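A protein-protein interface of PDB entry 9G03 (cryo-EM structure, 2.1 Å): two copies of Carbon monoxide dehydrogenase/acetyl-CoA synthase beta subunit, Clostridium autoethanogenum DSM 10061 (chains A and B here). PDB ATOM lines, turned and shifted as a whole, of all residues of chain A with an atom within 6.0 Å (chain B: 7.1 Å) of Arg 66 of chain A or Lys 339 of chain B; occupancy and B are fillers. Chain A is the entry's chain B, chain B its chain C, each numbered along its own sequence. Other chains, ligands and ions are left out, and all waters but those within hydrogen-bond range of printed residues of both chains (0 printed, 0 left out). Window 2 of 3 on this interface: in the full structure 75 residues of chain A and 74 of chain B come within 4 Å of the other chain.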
ATOM      1  N   CYS A  54      16.288  12.297  27.623  1.00  0.00           N
ATOM      2  CA  CYS A  54      17.237  12.013  26.554  1.00  0.00           C
ATOM      3  C   CYS A  54      16.496  11.950  25.227  1.00  0.00           C
ATOM      4  O   CYS A  54      15.441  11.318  25.128  1.00  0.00           O
ATOM      5  CB  CYS A  54      17.995  10.692  26.784  1.00  0.00           C
ATOM      6  SG  CYS A  54      19.050  10.589  28.259  1.00  0.00           S
ATOM      7  N   ARG A  55      17.054  12.599  24.217  1.00  0.00           N
ATOM      8  CA  ARG A  55      16.565  12.495  22.853  1.00  0.00           C
ATOM      9  C   ARG A  55      17.729  12.124  21.954  1.00  0.00           C
ATOM     10  O   ARG A  55      18.806  12.718  22.041  1.00  0.00           O
ATOM     11  CB  ARG A  55      15.882  13.788  22.385  1.00  0.00           C
ATOM     12  CG  ARG A  55      16.600  15.056  22.732  1.00  0.00           C
ATOM     13  CD  ARG A  55      15.698  16.252  22.545  1.00  0.00           C
ATOM     14  NE  ARG A  55      16.404  17.477  22.883  1.00  0.00           N
ATOM     15  CZ  ARG A  55      15.832  18.657  23.052  1.00  0.00           C
ATOM     16  NH1 ARG A  55      14.528  18.819  22.921  1.00  0.00           N
ATOM     17  NH2 ARG A  55      16.589  19.702  23.366  1.00  0.00           N
ATOM     18  N   VAL A  56      17.525  11.099  21.150  1.00  0.00           N
ATOM     19  CA  VAL A  56      18.515  10.646  20.195  1.00  0.00           C
ATOM     20  C   VAL A  56      17.975  10.914  18.799  1.00  0.00           C
ATOM     21  O   VAL A  56      16.771  11.084  18.589  1.00  0.00           O
ATOM     22  CB  VAL A  56      18.855   9.152  20.401  1.00  0.00           C
ATOM     23  CG1 VAL A  56      19.483   8.947  21.781  1.00  0.00           C
ATOM     24  CG2 VAL A  56      17.601   8.283  20.236  1.00  0.00           C
ATOM     25  N   VAL A  64      23.165  12.802  18.004  1.00  0.00           N
ATOM     26  CA  VAL A  64      23.325  12.006  19.215  1.00  0.00           C
ATOM     27  C   VAL A  64      22.743  10.618  18.997  1.00  0.00           C
ATOM     28  O   VAL A  64      21.595  10.468  18.571  1.00  0.00           O
ATOM     29  CB  VAL A  64      22.661  12.714  20.406  1.00  0.00           C
ATOM     30  CG1 VAL A  64      22.799  11.896  21.681  1.00  0.00           C
ATOM     31  CG2 VAL A  64      23.259  14.091  20.593  1.00  0.00           C
ATOM     32  N   GLU A  65      23.525   9.592  19.315  1.00  0.00           N
ATOM     33  CA  GLU A  65      23.126   8.215  19.057  1.00  0.00           C
ATOM     34  C   GLU A  65      22.526   7.526  20.274  1.00  0.00           C
ATOM     35  O   GLU A  65      21.619   6.710  20.119  1.00  0.00           O
ATOM     36  CB  GLU A  65      24.323   7.401  18.560  1.00  0.00           C
ATOM     37  CG  GLU A  65      25.121   8.061  17.448  1.00  0.00           C
ATOM     38  CD  GLU A  65      24.348   8.185  16.149  1.00  0.00           C
ATOM     39  OE1 GLU A  65      23.383   8.976  16.098  1.00  0.00           O
ATOM     40  OE2 GLU A  65      24.709   7.486  15.180  1.00  0.00           O
ATOM     41  N   ARG A  66      23.015   7.797  21.475  1.00  0.00           N
ATOM     42  CA  ARG A  66      22.583   7.056  22.648  1.00  0.00           C
ATOM     43  C   ARG A  66      22.139   8.003  23.744  1.00  0.00           C
ATOM     44  O   ARG A  66      22.646   9.119  23.864  1.00  0.00           O
ATOM     45  CB  ARG A  66      23.706   6.149  23.176  1.00  0.00           C
ATOM     46  CG  ARG A  66      24.136   5.064  22.193  1.00  0.00           C
ATOM     47  CD  ARG A  66      25.375   4.313  22.682  1.00  0.00           C
ATOM     48  NE  ARG A  66      25.662   3.138  21.866  1.00  0.00           N
ATOM     49  CZ  ARG A  66      25.349   1.888  22.183  1.00  0.00           C
ATOM     50  NH1 ARG A  66      24.762   1.584  23.331  1.00  0.00           N
ATOM     51  NH2 ARG A  66      25.649   0.912  21.333  1.00  0.00           N
ATOM     52  N   GLY A  67      21.204   7.533  24.560  1.00  0.00           N
ATOM     53  CA  GLY A  67      20.862   8.219  25.777  1.00  0.00           C
ATOM     54  C   GLY A  67      22.023   8.168  26.754  1.00  0.00           C
ATOM     55  O   GLY A  67      23.043   7.522  26.527  1.00  0.00           O
ATOM     56  N   ILE A  68      21.816   8.812  27.898  1.00  0.00           N
ATOM     57  CA  ILE A  68      22.879   8.945  28.892  1.00  0.00           C
ATOM     58  C   ILE A  68      23.297   7.580  29.426  1.00  0.00           C
ATOM     59  O   ILE A  68      24.487   7.304  29.580  1.00  0.00           O
ATOM     60  CB  ILE A  68      22.452   9.921  30.004  1.00  0.00           C
ATOM     61  CG1 ILE A  68      22.312  11.340  29.409  1.00  0.00           C
ATOM     62  CG2 ILE A  68      23.482   9.918  31.143  1.00  0.00           C
ATOM     63  CD1 ILE A  68      21.662  12.358  30.315  1.00  0.00           C
ATOM     64  N   GLY A  70      23.239   4.958  27.752  1.00  0.00           N
ATOM     65  CA  GLY A  70      23.720   4.222  26.602  1.00  0.00           C
ATOM     66  C   GLY A  70      22.659   3.574  25.736  1.00  0.00           C
ATOM     67  O   GLY A  70      23.013   2.875  24.790  1.00  0.00           O
ATOM     68  N   ALA A  71      21.383   3.798  26.015  1.00  0.00           N
ATOM     69  CA  ALA A  71      20.310   3.188  25.234  1.00  0.00           C
ATOM     70  C   ALA A  71      20.233   3.760  23.814  1.00  0.00           C
ATOM     71  O   ALA A  71      20.252   4.974  23.619  1.00  0.00           O
ATOM     72  CB  ALA A  71      18.980   3.396  25.959  1.00  0.00           C
ATOM     73  N   THR A  72      20.121   2.875  22.826  1.00  0.00           N
ATOM     74  CA  THR A  72      20.037   3.266  21.425  1.00  0.00           C
ATOM     75  C   THR A  72      18.629   3.736  21.075  1.00  0.00           C
ATOM     76  O   THR A  72      17.687   3.609  21.858  1.00  0.00           O
ATOM     77  CB  THR A  72      20.404   2.097  20.513  1.00  0.00           C
ATOM     78  OG1 THR A  72      19.510   1.008  20.771  1.00  0.00           O
ATOM     79  CG2 THR A  72      21.840   1.660  20.748  1.00  0.00           C
ATOM     80  N   ALA A  73      18.487   4.246  19.850  1.00  0.00           N
ATOM     81  CA  ALA A  73      17.170   4.651  19.373  1.00  0.00           C
ATOM     82  C   ALA A  73      16.210   3.469  19.347  1.00  0.00           C
ATOM     83  O   ALA A  73      15.059   3.595  19.767  1.00  0.00           O
ATOM     84  CB  ALA A  73      17.277   5.301  17.990  1.00  0.00           C
ATOM     85  N   ILE A  76      14.995   2.841  22.909  1.00  0.00           N
ATOM     86  CA  ILE A  76      14.060   3.865  23.380  1.00  0.00           C
ATOM     87  C   ILE A  76      12.698   3.690  22.715  1.00  0.00           C
ATOM     88  O   ILE A  76      11.654   3.716  23.381  1.00  0.00           O
ATOM     89  CB  ILE A  76      14.661   5.269  23.140  1.00  0.00           C
ATOM     90  CG1 ILE A  76      15.947   5.428  23.979  1.00  0.00           C
ATOM     91  CG2 ILE A  76      13.643   6.397  23.443  1.00  0.00           C
ATOM     92  CD1 ILE A  76      16.777   6.642  23.660  1.00  0.00           C
ATOM     93  N   VAL B  23      37.379   5.463  24.995  1.00  0.00           N
ATOM     94  CA  VAL B  23      36.035   4.957  25.242  1.00  0.00           C
ATOM     95  C   VAL B  23      35.233   6.046  25.936  1.00  0.00           C
ATOM     96  O   VAL B  23      35.777   6.887  26.659  1.00  0.00           O
ATOM     97  CB  VAL B  23      36.044   3.657  26.081  1.00  0.00           C
ATOM     98  CG1 VAL B  23      36.777   2.553  25.342  1.00  0.00           C
ATOM     99  CG2 VAL B  23      36.670   3.891  27.451  1.00  0.00           C
ATOM    100  N   GLU B  24      33.925   6.013  25.736  1.00  0.00           N
ATOM    101  CA  GLU B  24      33.047   7.017  26.309  1.00  0.00           C
ATOM    102  C   GLU B  24      32.327   6.476  27.533  1.00  0.00           C
ATOM    103  O   GLU B  24      31.985   5.295  27.607  1.00  0.00           O
ATOM    104  CB  GLU B  24      32.020   7.497  25.281  1.00  0.00           C
ATOM    105  CG  GLU B  24      30.900   6.527  25.028  1.00  0.00           C
ATOM    106  CD  GLU B  24      29.784   7.111  24.183  1.00  0.00           C
ATOM    107  OE1 GLU B  24      29.971   8.204  23.610  1.00  0.00           O
ATOM    108  OE2 GLU B  24      28.721   6.463  24.092  1.00  0.00           O
ATOM    109  N   ARG B  29      28.400  10.860  27.652  1.00  0.00           N
ATOM    110  CA  ARG B  29      27.072  10.882  27.051  1.00  0.00           C
ATOM    111  C   ARG B  29      26.223  12.000  27.646  1.00  0.00           C
ATOM    112  O   ARG B  29      25.479  12.664  26.923  1.00  0.00           O
ATOM    113  CB  ARG B  29      26.389   9.513  27.191  1.00  0.00           C
ATOM    114  CG  ARG B  29      27.080   8.401  26.380  1.00  0.00           C
ATOM    115  CD  ARG B  29      26.296   7.084  26.332  1.00  0.00           C
ATOM    116  NE  ARG B  29      26.074   6.491  27.647  1.00  0.00           N
ATOM    117  CZ  ARG B  29      26.975   5.793  28.332  1.00  0.00           C
ATOM    118  NH1 ARG B  29      28.195   5.590  27.869  1.00  0.00           N
ATOM    119  NH2 ARG B  29      26.643   5.302  29.522  1.00  0.00           N
ATOM    120  N   LYS B  30      26.359  12.256  28.947  1.00  0.00           N
ATOM    121  CA  LYS B  30      25.663  13.386  29.552  1.00  0.00           C
ATOM    122  C   LYS B  30      26.109  14.697  28.916  1.00  0.00           C
ATOM    123  O   LYS B  30      25.277  15.550  28.598  1.00  0.00           O
ATOM    124  CB  LYS B  30      25.894  13.418  31.066  1.00  0.00           C
ATOM    125  CG  LYS B  30      25.380  14.687  31.760  1.00  0.00           C
ATOM    126  CD  LYS B  30      23.864  14.795  31.666  1.00  0.00           C
ATOM    127  CE  LYS B  30      23.278  15.881  32.563  1.00  0.00           C
ATOM    128  NZ  LYS B  30      23.787  17.234  32.245  1.00  0.00           N
ATOM    129  N   ASP B  32      27.282  15.018  25.861  1.00  0.00           N
ATOM    130  CA  ASP B  32      26.757  15.019  24.498  1.00  0.00           C
ATOM    131  C   ASP B  32      25.284  15.400  24.468  1.00  0.00           C
ATOM    132  O   ASP B  32      24.825  16.019  23.504  1.00  0.00           O
ATOM    133  CB  ASP B  32      26.938  13.647  23.848  1.00  0.00           C
ATOM    134  CG  ASP B  32      28.381  13.267  23.682  1.00  0.00           C
ATOM    135  OD1 ASP B  32      29.225  14.177  23.556  1.00  0.00           O
ATOM    136  OD2 ASP B  32      28.677  12.058  23.683  1.00  0.00           O
ATOM    137  N   MET B  33      24.529  15.043  25.505  1.00  0.00           N
ATOM    138  CA  MET B  33      23.125  15.418  25.532  1.00  0.00           C
ATOM    139  C   MET B  33      22.938  16.925  25.654  1.00  0.00           C
ATOM    140  O   MET B  33      21.862  17.429  25.330  1.00  0.00           O
ATOM    141  CB  MET B  33      22.427  14.688  26.681  1.00  0.00           C
ATOM    142  CG  MET B  33      20.935  14.567  26.518  1.00  0.00           C
ATOM    143  SD  MET B  33      20.408  13.747  24.988  1.00  0.00           S
ATOM    144  CE  MET B  33      21.039  12.089  25.221  1.00  0.00           C
ATOM    145  N   MET B 334      23.667  -0.403  32.799  1.00  0.00           N
ATOM    146  CA  MET B 334      23.812   0.499  31.665  1.00  0.00           C
ATOM    147  C   MET B 334      24.000  -0.326  30.397  1.00  0.00           C
ATOM    148  O   MET B 334      24.928  -1.146  30.335  1.00  0.00           O
ATOM    149  CB  MET B 334      24.995   1.450  31.845  1.00  0.00           C
ATOM    150  CG  MET B 334      24.836   2.454  32.963  1.00  0.00           C
ATOM    151  SD  MET B 334      26.216   3.619  33.064  1.00  0.00           S
ATOM    152  CE  MET B 334      25.934   4.335  34.680  1.00  0.00           C
ATOM    153  N   PRO B 335      23.133  -0.181  29.390  1.00  0.00           N
ATOM    154  CA  PRO B 335      23.328  -0.964  28.161  1.00  0.00           C
ATOM    155  C   PRO B 335      24.647  -0.659  27.475  1.00  0.00           C
ATOM    156  O   PRO B 335      25.210  -1.540  26.818  1.00  0.00           O
ATOM    157  CB  PRO B 335      22.110  -0.587  27.300  1.00  0.00           C
ATOM    158  CG  PRO B 335      21.568   0.655  27.873  1.00  0.00           C
ATOM    159  CD  PRO B 335      21.894   0.621  29.336  1.00  0.00           C
ATOM    160  N   ALA B 336      25.199   0.538  27.668  1.00  0.00           N
ATOM    161  CA  ALA B 336      26.475   0.869  27.052  1.00  0.00           C
ATOM    162  C   ALA B 336      27.568  -0.120  27.430  1.00  0.00           C
ATOM    163  O   ALA B 336      28.534  -0.275  26.676  1.00  0.00           O
ATOM    164  CB  ALA B 336      26.902   2.281  27.460  1.00  0.00           C
ATOM    165  N   LEU B 337      27.424  -0.815  28.561  1.00  0.00           N
ATOM    166  CA  LEU B 337      28.410  -1.826  28.924  1.00  0.00           C
ATOM    167  C   LEU B 337      28.691  -2.767  27.762  1.00  0.00           C
ATOM    168  O   LEU B 337      29.852  -3.073  27.478  1.00  0.00           O
ATOM    169  CB  LEU B 337      27.930  -2.626  30.136  1.00  0.00           C
ATOM    170  CG  LEU B 337      28.015  -1.939  31.500  1.00  0.00           C
ATOM    171  CD1 LEU B 337      27.308  -2.775  32.554  1.00  0.00           C
ATOM    172  CD2 LEU B 337      29.464  -1.666  31.887  1.00  0.00           C
ATOM    173  N   ALA B 338      27.645  -3.204  27.050  1.00  0.00           N
ATOM    174  CA  ALA B 338      27.880  -4.102  25.926  1.00  0.00           C
ATOM    175  C   ALA B 338      28.883  -3.509  24.943  1.00  0.00           C
ATOM    176  O   ALA B 338      29.931  -4.105  24.672  1.00  0.00           O
ATOM    177  CB  ALA B 338      26.558  -4.404  25.216  1.00  0.00           C
ATOM    178  N   LYS B 339      28.629  -2.280  24.486  1.00  0.00           N
ATOM    179  CA  LYS B 339      29.575  -1.616  23.597  1.00  0.00           C
ATOM    180  C   LYS B 339      30.952  -1.521  24.245  1.00  0.00           C
ATOM    181  O   LYS B 339      31.962  -1.913  23.651  1.00  0.00           O
ATOM    182  CB  LYS B 339      29.045  -0.231  23.192  1.00  0.00           C
ATOM    183  CG  LYS B 339      29.932   0.532  22.196  1.00  0.00           C
ATOM    184  CD  LYS B 339      29.340   1.895  21.783  1.00  0.00           C
ATOM    185  CE  LYS B 339      30.249   2.648  20.806  1.00  0.00           C
ATOM    186  NZ  LYS B 339      29.706   3.976  20.379  1.00  0.00           N
ATOM    187  N   LEU B 340      30.989  -1.113  25.514  1.00  0.00           N
ATOM    188  CA  LEU B 340      32.265  -0.958  26.205  1.00  0.00           C
ATOM    189  C   LEU B 340      33.025  -2.275  26.264  1.00  0.00           C
ATOM    190  O   LEU B 340      34.246  -2.301  26.077  1.00  0.00           O
ATOM    191  CB  LEU B 340      32.035  -0.390  27.609  1.00  0.00           C
ATOM    192  CG  LEU B 340      33.273  -0.083  28.455  1.00  0.00           C
ATOM    193  CD1 LEU B 340      34.125   1.008  27.820  1.00  0.00           C
ATOM    194  CD2 LEU B 340      32.851   0.301  29.858  1.00  0.00           C
ATOM    195  N   SER B 341      32.307  -3.388  26.424  1.00  0.00           N
ATOM    196  CA  SER B 341      32.955  -4.690  26.543  1.00  0.00           C
ATOM    197  C   SER B 341      33.695  -5.087  25.276  1.00  0.00           C
ATOM    198  O   SER B 341      34.606  -5.915  25.340  1.00  0.00           O
ATOM    199  CB  SER B 341      31.928  -5.754  26.912  1.00  0.00           C
ATOM    200  OG  SER B 341      31.546  -5.618  28.260  1.00  0.00           O
ATOM    201  N   LYS B 342      33.371  -4.470  24.141  1.00  0.00           N
ATOM    202  CA  LYS B 342      34.086  -4.764  22.904  1.00  0.00           C
ATOM    203  C   LYS B 342      35.504  -4.211  22.931  1.00  0.00           C
ATOM    204  O   LYS B 342      36.386  -4.758  22.263  1.00  0.00           O
ATOM    205  CB  LYS B 342      33.326  -4.203  21.700  1.00  0.00           C
ATOM    206  CG  LYS B 342      31.847  -4.518  21.691  1.00  0.00           C
ATOM    207  CD  LYS B 342      31.574  -6.009  21.719  1.00  0.00           C
ATOM    208  CE  LYS B 342      30.151  -6.280  22.152  1.00  0.00           C
ATOM    209  NZ  LYS B 342      29.180  -5.404  21.447  1.00  0.00           N
ATOM    210  N   SER B 343      35.752  -3.152  23.696  1.00  0.00           N
ATOM    211  CA  SER B 343      37.076  -2.548  23.746  1.00  0.00           C
ATOM    212  C   SER B 343      38.032  -3.300  24.664  1.00  0.00           C
ATOM    213  O   SER B 343      39.213  -2.948  24.720  1.00  0.00           O
ATOM    214  CB  SER B 343      36.975  -1.093  24.207  1.00  0.00           C
ATOM    215  OG  SER B 343      36.304  -0.307  23.246  1.00  0.00           O
ATOM    216  N   TYR B 344      37.552  -4.322  25.372  1.00  0.00           N
ATOM    217  CA  TYR B 344      38.370  -5.122  26.267  1.00  0.00           C
ATOM    218  C   TYR B 344      38.016  -6.590  26.056  1.00  0.00           C
ATOM    219  O   TYR B 344      37.183  -6.932  25.212  1.00  0.00           O
ATOM    220  CB  TYR B 344      38.139  -4.702  27.725  1.00  0.00           C
ATOM    221  CG  TYR B 344      38.376  -3.232  27.971  1.00  0.00           C
ATOM    222  CD1 TYR B 344      39.628  -2.769  28.339  1.00  0.00           C
ATOM    223  CD2 TYR B 344      37.353  -2.304  27.816  1.00  0.00           C
ATOM    224  CE1 TYR B 344      39.857  -1.433  28.558  1.00  0.00           C
ATOM    225  CE2 TYR B 344      37.575  -0.959  28.034  1.00  0.00           C
ATOM    226  CZ  TYR B 344      38.834  -0.527  28.400  1.00  0.00           C
ATOM    227  OH  TYR B 344      39.063   0.811  28.618  1.00  0.00           O
ATOM    228  N   PHE B 348      30.623  -9.970  28.812  1.00  0.00           N
ATOM    229  CA  PHE B 348      29.444  -9.345  29.394  1.00  0.00           C
ATOM    230  C   PHE B 348      28.271 -10.313  29.259  1.00  0.00           C
ATOM    231  O   PHE B 348      27.783 -10.555  28.151  1.00  0.00           O
ATOM    232  CB  PHE B 348      29.179  -8.002  28.722  1.00  0.00           C
ATOM    233  CG  PHE B 348      27.997  -7.259  29.271  1.00  0.00           C
ATOM    234  CD1 PHE B 348      27.868  -7.045  30.629  1.00  0.00           C
ATOM    235  CD2 PHE B 348      27.022  -6.759  28.427  1.00  0.00           C
ATOM    236  CE1 PHE B 348      26.784  -6.364  31.136  1.00  0.00           C
ATOM    237  CE2 PHE B 348      25.934  -6.072  28.927  1.00  0.00           C
ATOM    238  CZ  PHE B 348      25.812  -5.878  30.286  1.00  0.00           C
ATOM    239  N   ILE B 357      20.081  -7.806  26.585  1.00  0.00           N
ATOM    240  CA  ILE B 357      20.851  -6.662  26.114  1.00  0.00           C
ATOM    241  C   ILE B 357      21.541  -7.041  24.810  1.00  0.00           C
ATOM    242  O   ILE B 357      22.298  -8.013  24.762  1.00  0.00           O
ATOM    243  CB  ILE B 357      21.879  -6.187  27.162  1.00  0.00           C
ATOM    244  CG1 ILE B 357      21.156  -5.819  28.467  1.00  0.00           C
ATOM    245  CG2 ILE B 357      22.681  -5.011  26.607  1.00  0.00           C
ATOM    246  CD1 ILE B 357      22.058  -5.320  29.574  1.00  0.00           C
ATOM    247  N   THR B 358      21.329  -6.232  23.775  1.00  0.00           N
ATOM    248  CA  THR B 358      21.864  -6.536  22.455  1.00  0.00           C
ATOM    249  C   THR B 358      23.386  -6.557  22.490  1.00  0.00           C
ATOM    250  O   THR B 358      24.028  -5.723  23.131  1.00  0.00           O
ATOM    251  CB  THR B 358      21.364  -5.500  21.435  1.00  0.00           C
ATOM    252  OG1 THR B 358      19.935  -5.449  21.464  1.00  0.00           O
ATOM    253  CG2 THR B 358      21.809  -5.858  20.023  1.00  0.00           C
ATOM    254  N   ASP B 359      23.959  -7.532  21.790  1.00  0.00           N
ATOM    255  CA  ASP B 359      25.394  -7.756  21.639  1.00  0.00           C
ATOM    256  C   ASP B 359      26.063  -8.232  22.924  1.00  0.00           C
ATOM    257  O   ASP B 359      27.293  -8.220  23.012  1.00  0.00           O
ATOM    258  CB  ASP B 359      26.113  -6.510  21.112  1.00  0.00           C
ATOM    259  CG  ASP B 359      25.680  -6.139  19.707  1.00  0.00           C
ATOM    260  OD1 ASP B 359      24.962  -6.942  19.073  1.00  0.00           O
ATOM    261  OD2 ASP B 359      26.054  -5.046  19.235  1.00  0.00           O
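Of the 21 printed residues of chain B, 7 touch a printed residue of chain A. Hydrophobic or aromatic side chains of chain A within 4 Å of the printed part of chain B: Val 64 and Ile 68.
No position is printed for both chains. Of the 14 pairs that touch across the chains among the printed residues, none has its exchanged pair printed and touching as well.
Among the printed residues, pairs that only touch across the chains: Cys 54 of chain A with Met 33 of chain B (3.7 Å), Val 64 of chain A with Asp 32 of chain B (3.8 Å), Val 64 of chain A with Met 33 of chain B (3.96 Å), Arg 66 of chain A with Met 33 of chain B (3.6 Å), Arg 66 of chain A with Lys 339 of chain B (3.8 Å), Gly 67 of chain A with Met 33 of chain B (3.9 Å), Ile 68 of chain A with Lys 30 of chain B (3.6 Å), Gly 70 of chain A with Pro 335 of chain B (3.8 Å), Gly 70 of chain A with Ala 336 of chain B (3.8 Å) and Ala 71 of chain A with Pro 335 of chain B (3.7 Å).
Of the printed residues of chain B, Arg 55 of chain A touches Met 33. Of the printed residues of chain B, Val 64 of chain A touches Asp 32 (3.8 Å) and Met 33 (3.96 Å). Gly 67 of chain A touches just these residues of chain B: Arg 29 (3.3 Å) and Met 33 (3.9 Å). Of the printed residues of chain B, Ile 68 of chain A touches Arg 29 and Lys 30. Printed residues of chain B within 4 Å of Gly 70 of chain A: Arg 29 (3.2 Å), Pro 335 (3.8 Å) and Ala 336 (3.8 Å). Thr 72 of chain A touches none of the printed residues of chain B. Of the printed residues of chain A, Asp 32 of chain B touches Val 64. Of chain A, only Arg 66 (3.8 Å) comes within 4 Å of Lys 339 of chain B. Ser 341 of chain B touches none of the printed residues of chain A. The nearest residue of chain B that does not touch Arg 66 of chain A is Ala 336 of chain B (4.2 Å). The nearest printed residue of chain B that does not touch Ala 71 of chain A is Ala 336 of chain B (5.3 Å).
The side-chain sulfur (SG) of Cys 54 of chain A lies close to the backbone NH (N) of Ile 68 of chain A. The guanidinium group (NH1) of Arg 66 of chain A is in hydrogen-bond range of the backbone carbonyl oxygen (O) of Gly 70 of chain A, 2.6 Å away. The side-chain carboxylate of Glu 24 of chain B lies within salt-bridge range of the guanidinium group of Arg 29 of chain B (3.9 Å).
The backbone NH (N) of Arg 55 of chain A lies within hydrogen-bond range of the side-chain sulfur (SD) of Met 33 of chain B (3.6 Å). O of Gly 67 of chain A lies close to NE of Arg 29 of chain B (3.4 Å). O of Ile 68 of chain A is in hydrogen-bond range of NE of Arg 29 of chain B, 2.6 Å away. The guanidinium group (NE) of Arg 29 of chain B sits close to the backbone NH (N) of Gly 70 of chain A (3.2 Å).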
